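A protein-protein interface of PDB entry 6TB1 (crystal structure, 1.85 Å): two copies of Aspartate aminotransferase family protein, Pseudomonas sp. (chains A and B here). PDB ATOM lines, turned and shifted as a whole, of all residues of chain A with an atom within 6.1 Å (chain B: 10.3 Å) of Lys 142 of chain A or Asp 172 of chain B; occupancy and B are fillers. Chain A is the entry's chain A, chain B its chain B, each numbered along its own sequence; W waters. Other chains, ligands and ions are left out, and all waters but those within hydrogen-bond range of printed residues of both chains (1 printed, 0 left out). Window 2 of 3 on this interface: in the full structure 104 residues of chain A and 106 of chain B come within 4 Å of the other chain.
Of the 18 printed residues of chain A, 4 touch a printed residue of chain B. Printed residues of chain A that touch a printed residue of chain B: Trp 130, Tyr 131, Asn 134 and Lys 142. Hydrophobic or aromatic side chains of chain A that line the printed part of chain B: Trp 130 and Tyr 131. Printed residues of chain B that touch a printed residue of chain A: Gly 170, Phe 171 and Asp 172. Hydrophobic or aromatic side chains of chain B within 4 Å of the printed part of chain A: Phe 171. Among the printed residues, 6 pairs touch across the chains.
1 position is printed for both chains. Of the 6 pairs that touch across the chains among the printed residues, none has its exchanged pair printed and touching as well.
O of Gly 170 of chain B lies within hydrogen-bond range of ND2 of Asn 134 of chain A. The side-chain amide nitrogen (ND2) of Asn 134 of chain A is in hydrogen-bond range of the side-chain carboxylate (OD1) of Asp 172 of chain B (3.0 Å). NZ of Lys 142 of chain A is in salt-bridge range of OD2 of Asp 172 of chain B (2.8 Å).
The backbone carbonyl oxygen (O) of Trp 130 of chain A is in hydrogen-bond range of the side-chain amide nitrogen (ND2) of Asn 134 of chain A (3.3 Å). The indole nitrogen (NE1) of Trp 130 of chain A sits at hydrogen-bond distance from the backbone carbonyl oxygen (O) of Lys 142 of chain A (2.9 Å). The side-chain amino group of Lys 142 of chain A is in hydrogen-bond range of the side-chain amide oxygen of Asn 134 of chain A (2.9 Å). The side-chain amino group of Lys 142 of chain A lies within hydrogen-bond range of the backbone carbonyl oxygen of Pro 139 of chain A (2.8 Å). N of Lys 142 of chain A sits at hydrogen-bond distance from O of Thr 218 of chain A.
Printed residues of chain B within 4 Å of Trp 130 of chain A: Phe 171. Of the printed residues of chain B, Tyr 131 of chain A touches Gly 170 and Phe 171. Printed residues of chain B within 4 Å of Asn 134 of chain A: Gly 170 (2.9 Å) and Asp 172 (3.0 Å). No residue of chain B comes within 4 Å of Pro 139 of chain A. Of chain B, only Asp 172 comes within 4 Å of Lys 142 of chain A. Of the printed residues of chain A, Gly 170 of chain B touches Tyr 131 and Asn 134. Printed residues of chain A within 4 Å of Phe 171 of chain B: Trp 130 (3.3 Å) and Tyr 131 (3.3 Å). Of chain A, only Asn 134 (3.0 Å) and Lys 142 (2.8 Å) come within 4 Å of Asp 172 of chain B. The nearest printed residue of chain A that does not touch Phe 171 of chain B is Asn 134 of chain A (4.4 Å).
Trp 130 of chain A touches Phe 171 of chain B (CE3 to O, 3.3 Å). Tyr 131 of chain A touches Gly 170 of chain B (CA to O, 3.3 Å). Phe 171 of chain B touches Tyr 131 of chain A (CE1 to CD1, 3.3 Å).
Water W1 lies within hydrogen-bond range of the side-chain carboxylate of Asp 172 of chain B (3.0 Å), the side-chain amino group of Lys 142 of chain A (3.1 Å) and the side-chain amide oxygen of Asn 134 of chain A (3.5 Å).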
ATOM      1  N   VAL A 129      11.410 -14.783  20.759  1.00  0.00           N
ATOM      2  CA  VAL A 129      10.873 -16.010  21.418  1.00  0.00           C
ATOM      3  C   VAL A 129      10.536 -17.060  20.341  1.00  0.00           C
ATOM      4  O   VAL A 129      10.898 -18.226  20.542  1.00  0.00           O
ATOM      5  CB  VAL A 129       9.694 -15.691  22.347  1.00  0.00           C
ATOM      6  CG1 VAL A 129       8.983 -16.956  22.812  1.00  0.00           C
ATOM      7  CG2 VAL A 129      10.136 -14.877  23.553  1.00  0.00           C
ATOM      8  N   TRP A 130       9.913 -16.667  19.223  1.00  0.00           N
ATOM      9  CA  TRP A 130       9.678 -17.556  18.052  1.00  0.00           C
ATOM     10  C   TRP A 130      11.013 -18.113  17.531  1.00  0.00           C
ATOM     11  O   TRP A 130      11.092 -19.345  17.276  1.00  0.00           O
ATOM     12  CB  TRP A 130       8.872 -16.834  16.958  1.00  0.00           C
ATOM     13  CG  TRP A 130       7.456 -16.483  17.333  1.00  0.00           C
ATOM     14  CD1 TRP A 130       6.765 -16.853  18.456  1.00  0.00           C
ATOM     15  CD2 TRP A 130       6.547 -15.667  16.567  1.00  0.00           C
ATOM     16  NE1 TRP A 130       5.500 -16.327  18.440  1.00  0.00           N
ATOM     17  CE2 TRP A 130       5.333 -15.607  17.285  1.00  0.00           C
ATOM     18  CE3 TRP A 130       6.647 -14.983  15.348  1.00  0.00           C
ATOM     19  CZ2 TRP A 130       4.227 -14.898  16.816  1.00  0.00           C
ATOM     20  CZ3 TRP A 130       5.548 -14.290  14.881  1.00  0.00           C
ATOM     21  CH2 TRP A 130       4.362 -14.230  15.618  1.00  0.00           C
ATOM     22  N   TYR A 131      12.029 -17.259  17.381  1.00  0.00           N
ATOM     23  CA  TYR A 131      13.390 -17.604  16.867  1.00  0.00           C
ATOM     24  C   TYR A 131      14.046 -18.627  17.809  1.00  0.00           C
ATOM     25  O   TYR A 131      14.575 -19.646  17.319  1.00  0.00           O
ATOM     26  CB  TYR A 131      14.198 -16.309  16.761  1.00  0.00           C
ATOM     27  CG  TYR A 131      15.489 -16.276  15.986  1.00  0.00           C
ATOM     28  CD1 TYR A 131      15.489 -16.156  14.603  1.00  0.00           C
ATOM     29  CD2 TYR A 131      16.702 -16.153  16.647  1.00  0.00           C
ATOM     30  CE1 TYR A 131      16.668 -16.004  13.886  1.00  0.00           C
ATOM     31  CE2 TYR A 131      17.893 -16.007  15.947  1.00  0.00           C
ATOM     32  CZ  TYR A 131      17.872 -15.930  14.565  1.00  0.00           C
ATOM     33  OH  TYR A 131      19.024 -15.770  13.858  1.00  0.00           O
ATOM     34  N   ASN A 133      12.576 -20.740  20.095  1.00  0.00           N
ATOM     35  CA  ASN A 133      11.867 -22.045  20.136  1.00  0.00           C
ATOM     36  C   ASN A 133      12.091 -22.804  18.817  1.00  0.00           C
ATOM     37  O   ASN A 133      12.252 -24.041  18.885  1.00  0.00           O
ATOM     38  CB  ASN A 133      10.414 -21.873  20.599  1.00  0.00           C
ATOM     39  CG  ASN A 133      10.360 -21.694  22.104  1.00  0.00           C
ATOM     40  OD1 ASN A 133      11.239 -22.182  22.808  1.00  0.00           O
ATOM     41  ND2 ASN A 133       9.387 -20.953  22.605  1.00  0.00           N
ATOM     42  N   ASN A 134      12.205 -22.113  17.676  1.00  0.00           N
ATOM     43  CA  ASN A 134      12.661 -22.744  16.409  1.00  0.00           C
ATOM     44  C   ASN A 134      14.080 -23.305  16.597  1.00  0.00           C
ATOM     45  O   ASN A 134      14.295 -24.464  16.192  1.00  0.00           O
ATOM     46  CB  ASN A 134      12.561 -21.800  15.209  1.00  0.00           C
ATOM     47  CG  ASN A 134      11.147 -21.626  14.695  1.00  0.00           C
ATOM     48  OD1 ASN A 134      10.329 -22.546  14.756  1.00  0.00           O
ATOM     49  ND2 ASN A 134      10.842 -20.445  14.178  1.00  0.00           N
ATOM     50  N   LYS A 138      11.469 -26.733  18.966  1.00  0.00           N
ATOM     51  CA  LYS A 138      10.078 -26.746  19.492  1.00  0.00           C
ATOM     52  C   LYS A 138       9.211 -25.841  18.629  1.00  0.00           C
ATOM     53  O   LYS A 138       8.757 -24.793  19.093  1.00  0.00           O
ATOM     54  CB  LYS A 138      10.076 -26.299  20.953  1.00  0.00           C
ATOM     55  CG  LYS A 138      11.036 -27.043  21.862  1.00  0.00           C
ATOM     56  CD  LYS A 138      11.035 -26.455  23.236  1.00  0.00           C
ATOM     57  CE  LYS A 138      12.224 -26.876  24.061  1.00  0.00           C
ATOM     58  NZ  LYS A 138      12.352 -26.003  25.252  1.00  0.00           N
ATOM     59  N   PRO A 139       8.961 -26.211  17.352  1.00  0.00           N
ATOM     60  CA  PRO A 139       8.253 -25.332  16.424  1.00  0.00           C
ATOM     61  C   PRO A 139       6.793 -25.016  16.784  1.00  0.00           C
ATOM     62  O   PRO A 139       6.300 -24.050  16.251  1.00  0.00           O
ATOM     63  CB  PRO A 139       8.320 -26.077  15.086  1.00  0.00           C
ATOM     64  CG  PRO A 139       8.517 -27.518  15.472  1.00  0.00           C
ATOM     65  CD  PRO A 139       9.374 -27.475  16.716  1.00  0.00           C
ATOM     66  N   ALA A 140       6.143 -25.793  17.656  1.00  0.00           N
ATOM     67  CA  ALA A 140       4.751 -25.534  18.105  1.00  0.00           C
ATOM     68  C   ALA A 140       4.712 -24.534  19.279  1.00  0.00           C
ATOM     69  O   ALA A 140       3.629 -24.025  19.550  1.00  0.00           O
ATOM     70  CB  ALA A 140       4.077 -26.833  18.497  1.00  0.00           C
ATOM     71  N   LYS A 141       5.826 -24.301  19.981  1.00  0.00           N
ATOM     72  CA  LYS A 141       5.848 -23.520  21.250  1.00  0.00           C
ATOM     73  C   LYS A 141       5.976 -22.027  20.898  1.00  0.00           C
ATOM     74  O   LYS A 141       7.118 -21.501  20.946  1.00  0.00           O
ATOM     75  CB  LYS A 141       6.974 -24.029  22.154  1.00  0.00           C
ATOM     76  CG  LYS A 141       6.882 -23.630  23.624  1.00  0.00           C
ATOM     77  CD  LYS A 141       7.942 -24.306  24.474  1.00  0.00           C
ATOM     78  CE  LYS A 141       7.929 -23.938  25.946  1.00  0.00           C
ATOM     79  NZ  LYS A 141       6.664 -24.336  26.616  1.00  0.00           N
ATOM     80  N   LYS A 142       4.851 -21.391  20.551  1.00  0.00           N
ATOM     81  CA  LYS A 142       4.811 -20.040  19.909  1.00  0.00           C
ATOM     82  C   LYS A 142       3.744 -19.108  20.504  1.00  0.00           C
ATOM     83  O   LYS A 142       3.841 -17.876  20.251  1.00  0.00           O
ATOM     84  CB  LYS A 142       4.557 -20.174  18.403  1.00  0.00           C
ATOM     85  CG  LYS A 142       5.600 -20.976  17.637  1.00  0.00           C
ATOM     86  CD  LYS A 142       7.018 -20.443  17.744  1.00  0.00           C
ATOM     87  CE  LYS A 142       8.048 -21.379  17.140  1.00  0.00           C
ATOM     88  NZ  LYS A 142       7.745 -21.693  15.726  1.00  0.00           N
ATOM     89  N   LYS A 143       2.759 -19.617  21.247  1.00  0.00           N
ATOM     90  CA  LYS A 143       1.612 -18.800  21.714  1.00  0.00           C
ATOM     91  C   LYS A 143       2.043 -17.904  22.889  1.00  0.00           C
ATOM     92  O   LYS A 143       2.897 -18.327  23.731  1.00  0.00           O
ATOM     93  CB  LYS A 143       0.420 -19.685  22.088  1.00  0.00           C
ATOM     94  CG  LYS A 143      -0.188 -20.491  20.944  1.00  0.00           C
ATOM     95  CD  LYS A 143      -1.310 -21.417  21.430  1.00  0.00           C
ATOM     96  CE  LYS A 143      -1.883 -22.333  20.358  1.00  0.00           C
ATOM     97  NZ  LYS A 143      -2.452 -23.571  20.953  1.00  0.00           N
ATOM     98  N   PHE A 144       1.480 -16.695  22.944  1.00  0.00           N
ATOM     99  CA  PHE A 144       1.694 -15.718  24.045  1.00  0.00           C
ATOM    100  C   PHE A 144       0.402 -15.607  24.861  1.00  0.00           C
ATOM    101  O   PHE A 144      -0.683 -15.587  24.266  1.00  0.00           O
ATOM    102  CB  PHE A 144       2.117 -14.342  23.500  1.00  0.00           C
ATOM    103  CG  PHE A 144       3.606 -14.166  23.337  1.00  0.00           C
ATOM    104  CD1 PHE A 144       4.290 -14.812  22.320  1.00  0.00           C
ATOM    105  CD2 PHE A 144       4.320 -13.318  24.173  1.00  0.00           C
ATOM    106  CE1 PHE A 144       5.663 -14.664  22.180  1.00  0.00           C
ATOM    107  CE2 PHE A 144       5.692 -13.171  24.027  1.00  0.00           C
ATOM    108  CZ  PHE A 144       6.360 -13.839  23.028  1.00  0.00           C
ATOM    109  N   GLY A 177      -3.060 -16.747  18.072  1.00  0.00           N
ATOM    110  CA  GLY A 177      -1.943 -17.215  18.918  1.00  0.00           C
ATOM    111  C   GLY A 177      -1.574 -16.217  20.009  1.00  0.00           C
ATOM    112  O   GLY A 177      -0.552 -16.446  20.704  1.00  0.00           O
ATOM    113  N   GLU A 217       2.648 -27.575  25.428  1.00  0.00           N
ATOM    114  CA  GLU A 217       3.772 -27.618  24.459  1.00  0.00           C
ATOM    115  C   GLU A 217       3.610 -26.483  23.432  1.00  0.00           C
ATOM    116  O   GLU A 217       4.571 -26.256  22.686  1.00  0.00           O
ATOM    117  CB  GLU A 217       3.863 -29.012  23.813  1.00  0.00           C
ATOM    118  CG  GLU A 217       2.782 -29.325  22.781  1.00  0.00           C
ATOM    119  CD  GLU A 217       1.373 -29.613  23.285  1.00  0.00           C
ATOM    120  OE1 GLU A 217       1.193 -29.753  24.525  1.00  0.00           O
ATOM    121  OE2 GLU A 217       0.451 -29.686  22.437  1.00  0.00           O
ATOM    122  N   THR A 218       2.447 -25.814  23.373  1.00  0.00           N
ATOM    123  CA  THR A 218       2.173 -24.714  22.406  1.00  0.00           C
ATOM    124  C   THR A 218       2.383 -23.324  23.039  1.00  0.00           C
ATOM    125  O   THR A 218       2.280 -22.349  22.286  1.00  0.00           O
ATOM    126  CB  THR A 218       0.770 -24.822  21.790  1.00  0.00           C
ATOM    127  OG1 THR A 218      -0.218 -24.498  22.768  1.00  0.00           O
ATOM    128  CG2 THR A 218       0.485 -26.181  21.188  1.00  0.00           C
ATOM    129  N   ILE A 219       2.616 -23.224  24.351  1.00  0.00           N
ATOM    130  CA  ILE A 219       2.678 -21.925  25.093  1.00  0.00           C
ATOM    131  C   ILE A 219       4.153 -21.548  25.300  1.00  0.00           C
ATOM    132  O   ILE A 219       4.871 -22.265  26.048  1.00  0.00           O
ATOM    133  CB  ILE A 219       1.918 -21.974  26.440  1.00  0.00           C
ATOM    134  CG1 ILE A 219       0.468 -22.455  26.300  1.00  0.00           C
ATOM    135  CG2 ILE A 219       2.001 -20.628  27.156  1.00  0.00           C
ATOM    136  CD1 ILE A 219      -0.395 -21.681  25.336  1.00  0.00           C
ATOM    137  N   ALA A 220       4.582 -20.432  24.698  1.00  0.00           N
ATOM    138  CA  ALA A 220       5.982 -19.941  24.756  1.00  0.00           C
ATOM    139  C   ALA A 220       6.197 -19.013  25.961  1.00  0.00           C
ATOM    140  O   ALA A 220       7.272 -19.108  26.626  1.00  0.00           O
ATOM    141  CB  ALA A 220       6.327 -19.263  23.457  1.00  0.00           C
ATOM    142  N   ALA A 221       5.260 -18.097  26.238  1.00  0.00           N
ATOM    143  CA  ALA A 221       5.548 -16.972  27.155  1.00  0.00           C
ATOM    144  C   ALA A 221       4.284 -16.364  27.762  1.00  0.00           C
ATOM    145  O   ALA A 221       3.223 -16.372  27.096  1.00  0.00           O
ATOM    146  CB  ALA A 221       6.350 -15.929  26.404  1.00  0.00           C
ATOM    147  N   THR B 155       9.354  -5.183  12.003  1.00  0.00           N
ATOM    148  CA  THR B 155       8.280  -5.631  12.946  1.00  0.00           C
ATOM    149  C   THR B 155       7.650  -6.928  12.390  1.00  0.00           C
ATOM    150  O   THR B 155       7.846  -7.244  11.207  1.00  0.00           O
ATOM    151  CB  THR B 155       7.225  -4.556  13.244  1.00  0.00           C
ATOM    152  OG1 THR B 155       6.473  -4.309  12.044  1.00  0.00           O
ATOM    153  CG2 THR B 155       7.841  -3.269  13.784  1.00  0.00           C
ATOM    154  N   VAL B 156       6.879  -7.650  13.202  1.00  0.00           N
ATOM    155  CA  VAL B 156       6.159  -8.872  12.728  1.00  0.00           C
ATOM    156  C   VAL B 156       5.433  -8.537  11.411  1.00  0.00           C
ATOM    157  O   VAL B 156       5.628  -9.279  10.443  1.00  0.00           O
ATOM    158  CB  VAL B 156       5.214  -9.431  13.803  1.00  0.00           C
ATOM    159  CG1 VAL B 156       4.297 -10.507  13.245  1.00  0.00           C
ATOM    160  CG2 VAL B 156       5.997  -9.945  14.999  1.00  0.00           C
ATOM    161  N   ALA B 157       4.693  -7.430  11.321  1.00  0.00           N
ATOM    162  CA  ALA B 157       3.982  -7.045  10.070  1.00  0.00           C
ATOM    163  C   ALA B 157       4.938  -6.478   8.998  1.00  0.00           C
ATOM    164  O   ALA B 157       4.838  -6.893   7.820  1.00  0.00           O
ATOM    165  CB  ALA B 157       2.860  -6.087  10.384  1.00  0.00           C
ATOM    166  N   ALA B 159       8.198  -6.864   8.503  1.00  0.00           N
ATOM    167  CA  ALA B 159       9.071  -7.970   8.030  1.00  0.00           C
ATOM    168  C   ALA B 159       8.282  -8.971   7.172  1.00  0.00           C
ATOM    169  O   ALA B 159       8.932  -9.709   6.400  1.00  0.00           O
ATOM    170  CB  ALA B 159       9.745  -8.662   9.198  1.00  0.00           C
ATOM    171  N   SER B 160       6.948  -8.997   7.279  1.00  0.00           N
ATOM    172  CA  SER B 160       6.066  -9.776   6.364  1.00  0.00           C
ATOM    173  C   SER B 160       5.964  -9.058   5.013  1.00  0.00           C
ATOM    174  O   SER B 160       5.916  -9.745   3.989  1.00  0.00           O
ATOM    175  CB  SER B 160       4.714 -10.056   6.991  1.00  0.00           C
ATOM    176  OG  SER B 160       4.875 -10.865   8.150  1.00  0.00           O
ATOM    177  N   PRO B 165      14.569 -13.078   2.335  1.00  0.00           N
ATOM    178  CA  PRO B 165      14.450 -14.260   3.194  1.00  0.00           C
ATOM    179  C   PRO B 165      15.200 -14.177   4.536  1.00  0.00           C
ATOM    180  O   PRO B 165      14.731 -14.760   5.484  1.00  0.00           O
ATOM    181  CB  PRO B 165      15.029 -15.392   2.312  1.00  0.00           C
ATOM    182  CG  PRO B 165      14.824 -14.902   0.890  1.00  0.00           C
ATOM    183  CD  PRO B 165      15.025 -13.401   0.966  1.00  0.00           C
ATOM    184  N   GLY B 166      16.342 -13.489   4.591  1.00  0.00           N
ATOM    185  CA  GLY B 166      17.119 -13.257   5.829  1.00  0.00           C
ATOM    186  C   GLY B 166      16.307 -12.563   6.915  1.00  0.00           C
ATOM    187  O   GLY B 166      16.614 -12.767   8.098  1.00  0.00           O
ATOM    188  N   ASN B 167      15.276 -11.790   6.552  1.00  0.00           N
ATOM    189  CA  ASN B 167      14.371 -11.116   7.519  1.00  0.00           C
ATOM    190  C   ASN B 167      13.227 -12.042   7.962  1.00  0.00           C
ATOM    191  O   ASN B 167      12.453 -11.634   8.850  1.00  0.00           O
ATOM    192  CB  ASN B 167      13.866  -9.798   6.925  1.00  0.00           C
ATOM    193  CG  ASN B 167      14.935  -8.722   6.961  1.00  0.00           C
ATOM    194  OD1 ASN B 167      15.240  -8.180   8.034  1.00  0.00           O
ATOM    195  ND2 ASN B 167      15.514  -8.412   5.816  1.00  0.00           N
ATOM    196  N   GLN B 168      13.092 -13.243   7.381  1.00  0.00           N
ATOM    197  CA  GLN B 168      11.879 -14.096   7.592  1.00  0.00           C
ATOM    198  C   GLN B 168      12.255 -15.484   8.135  1.00  0.00           C
ATOM    199  O   GLN B 168      11.538 -15.990   9.024  1.00  0.00           O
ATOM    200  CB  GLN B 168      11.082 -14.187   6.291  1.00  0.00           C
ATOM    201  CG  GLN B 168      10.630 -12.828   5.780  1.00  0.00           C
ATOM    202  CD  GLN B 168       9.746 -12.911   4.567  1.00  0.00           C
ATOM    203  OE1 GLN B 168       9.874 -13.798   3.727  1.00  0.00           O
ATOM    204  NE2 GLN B 168       8.847 -11.951   4.440  1.00  0.00           N
ATOM    205  N   ARG B 169      13.344 -16.078   7.637  1.00  0.00           N
ATOM    206  CA  ARG B 169      13.808 -17.440   8.020  1.00  0.00           C
ATOM    207  C   ARG B 169      14.026 -17.501   9.535  1.00  0.00           C
ATOM    208  O   ARG B 169      14.822 -16.698  10.063  1.00  0.00           O
ATOM    209  CB  ARG B 169      15.073 -17.775   7.218  1.00  0.00           C
ATOM    210  CG  ARG B 169      15.536 -19.220   7.307  1.00  0.00           C
ATOM    211  CD  ARG B 169      16.808 -19.457   6.489  1.00  0.00           C
ATOM    212  NE  ARG B 169      16.652 -19.308   5.039  1.00  0.00           N
ATOM    213  CZ  ARG B 169      17.136 -18.310   4.275  1.00  0.00           C
ATOM    214  NH1 ARG B 169      16.929 -18.336   2.967  1.00  0.00           N
ATOM    215  NH2 ARG B 169      17.812 -17.293   4.796  1.00  0.00           N
ATOM    216  N   GLY B 170      13.334 -18.421  10.215  1.00  0.00           N
ATOM    217  CA  GLY B 170      13.454 -18.627  11.668  1.00  0.00           C
ATOM    218  C   GLY B 170      12.463 -17.809  12.474  1.00  0.00           C
ATOM    219  O   GLY B 170      12.407 -18.026  13.702  1.00  0.00           O
ATOM    220  N   PHE B 171      11.730 -16.878  11.837  1.00  0.00           N
ATOM    221  CA  PHE B 171      10.817 -15.920  12.526  1.00  0.00           C
ATOM    222  C   PHE B 171       9.349 -16.257  12.227  1.00  0.00           C
ATOM    223  O   PHE B 171       8.480 -15.463  12.664  1.00  0.00           O
ATOM    224  CB  PHE B 171      11.122 -14.467  12.124  1.00  0.00           C
ATOM    225  CG  PHE B 171      12.444 -13.926  12.606  1.00  0.00           C
ATOM    226  CD1 PHE B 171      12.694 -13.776  13.963  1.00  0.00           C
ATOM    227  CD2 PHE B 171      13.424 -13.538  11.709  1.00  0.00           C
ATOM    228  CE1 PHE B 171      13.903 -13.268  14.410  1.00  0.00           C
ATOM    229  CE2 PHE B 171      14.632 -13.020  12.154  1.00  0.00           C
ATOM    230  CZ  PHE B 171      14.871 -12.888  13.502  1.00  0.00           C
ATOM    231  N   ASP B 172       9.069 -17.364  11.513  1.00  0.00           N
ATOM    232  CA  ASP B 172       7.693 -17.811  11.145  1.00  0.00           C
ATOM    233  C   ASP B 172       6.979 -16.748  10.293  1.00  0.00           C
ATOM    234  O   ASP B 172       5.750 -16.604  10.427  1.00  0.00           O
ATOM    235  CB  ASP B 172       6.850 -18.143  12.384  1.00  0.00           C
ATOM    236  CG  ASP B 172       7.378 -19.270  13.258  1.00  0.00           C
ATOM    237  OD1 ASP B 172       8.249 -20.019  12.798  1.00  0.00           O
ATOM    238  OD2 ASP B 172       6.920 -19.378  14.417  1.00  0.00           O
ATOM    239  N   LEU B 173       7.704 -16.050   9.417  1.00  0.00           N
ATOM    240  CA  LEU B 173       7.144 -14.985   8.555  1.00  0.00           C
ATOM    241  C   LEU B 173       7.281 -15.411   7.098  1.00  0.00           C
ATOM    242  O   LEU B 173       8.149 -16.205   6.762  1.00  0.00           O
ATOM    243  CB  LEU B 173       7.890 -13.672   8.830  1.00  0.00           C
ATOM    244  CG  LEU B 173       7.848 -13.169  10.269  1.00  0.00           C
ATOM    245  CD1 LEU B 173       8.571 -11.837  10.393  1.00  0.00           C
ATOM    246  CD2 LEU B 173       6.418 -13.034  10.787  1.00  0.00           C
ATOM    247  N   PRO B 174       6.468 -14.886   6.157  1.00  0.00           N
ATOM    248  CA  PRO B 174       5.454 -13.874   6.450  1.00  0.00           C
ATOM    249  C   PRO B 174       4.182 -14.401   7.121  1.00  0.00           C
ATOM    250  O   PRO B 174       3.879 -15.584   6.971  1.00  0.00           O
ATOM    251  CB  PRO B 174       5.076 -13.380   5.053  1.00  0.00           C
ATOM    252  CG  PRO B 174       5.291 -14.589   4.155  1.00  0.00           C
ATOM    253  CD  PRO B 174       6.512 -15.258   4.734  1.00  0.00           C
ATOM    254  N   LEU B 175       3.455 -13.512   7.796  1.00  0.00           N
ATOM    255  CA  LEU B 175       2.062 -13.760   8.252  1.00  0.00           C
ATOM    256  C   LEU B 175       1.209 -14.084   7.026  1.00  0.00           C
ATOM    257  O   LEU B 175       1.495 -13.624   5.921  1.00  0.00           O
ATOM    258  CB  LEU B 175       1.478 -12.516   8.941  1.00  0.00           C
ATOM    259  CG  LEU B 175       2.091 -12.051  10.267  1.00  0.00           C
ATOM    260  CD1 LEU B 175       1.388 -10.786  10.730  1.00  0.00           C
ATOM    261  CD2 LEU B 175       2.012 -13.111  11.345  1.00  0.00           C
ATOM    262  N   PRO B 176       0.073 -14.798   7.210  1.00  0.00           N
ATOM    263  CA  PRO B 176      -0.981 -14.865   6.198  1.00  0.00           C
ATOM    264  C   PRO B 176      -1.486 -13.492   5.714  1.00  0.00           C
ATOM    265  O   PRO B 176      -1.640 -12.594   6.524  1.00  0.00           O
ATOM    266  CB  PRO B 176      -2.144 -15.578   6.937  1.00  0.00           C
ATOM    267  CG  PRO B 176      -1.496 -16.341   8.071  1.00  0.00           C
ATOM    268  CD  PRO B 176      -0.237 -15.567   8.425  1.00  0.00           C
ATOM    269  N   GLY B 177      -1.771 -13.364   4.416  1.00  0.00           N
ATOM    270  CA  GLY B 177      -2.370 -12.156   3.818  1.00  0.00           C
ATOM    271  C   GLY B 177      -1.316 -11.162   3.351  1.00  0.00           C
ATOM    272  O   GLY B 177      -1.687 -10.063   2.947  1.00  0.00           O
ATOM    273  N   PHE B 178      -0.035 -11.546   3.424  1.00  0.00           N
ATOM    274  CA  PHE B 178       1.139 -10.766   2.949  1.00  0.00           C
ATOM    275  C   PHE B 178       1.767 -11.541   1.783  1.00  0.00           C
ATOM    276  O   PHE B 178       2.489 -12.514   2.031  1.00  0.00           O
ATOM    277  CB  PHE B 178       2.101 -10.505   4.116  1.00  0.00           C
ATOM    278  CG  PHE B 178       1.542  -9.597   5.183  1.00  0.00           C
ATOM    279  CD1 PHE B 178       0.726 -10.090   6.195  1.00  0.00           C
ATOM    280  CD2 PHE B 178       1.814  -8.238   5.167  1.00  0.00           C
ATOM    281  CE1 PHE B 178       0.206  -9.248   7.169  1.00  0.00           C
ATOM    282  CE2 PHE B 178       1.281  -7.398   6.135  1.00  0.00           C
ATOM    283  CZ  PHE B 178       0.474  -7.897   7.129  1.00  0.00           C
HETATM  284  O   HOH W   1       7.392 -22.872  12.884  1.00  0.00           O
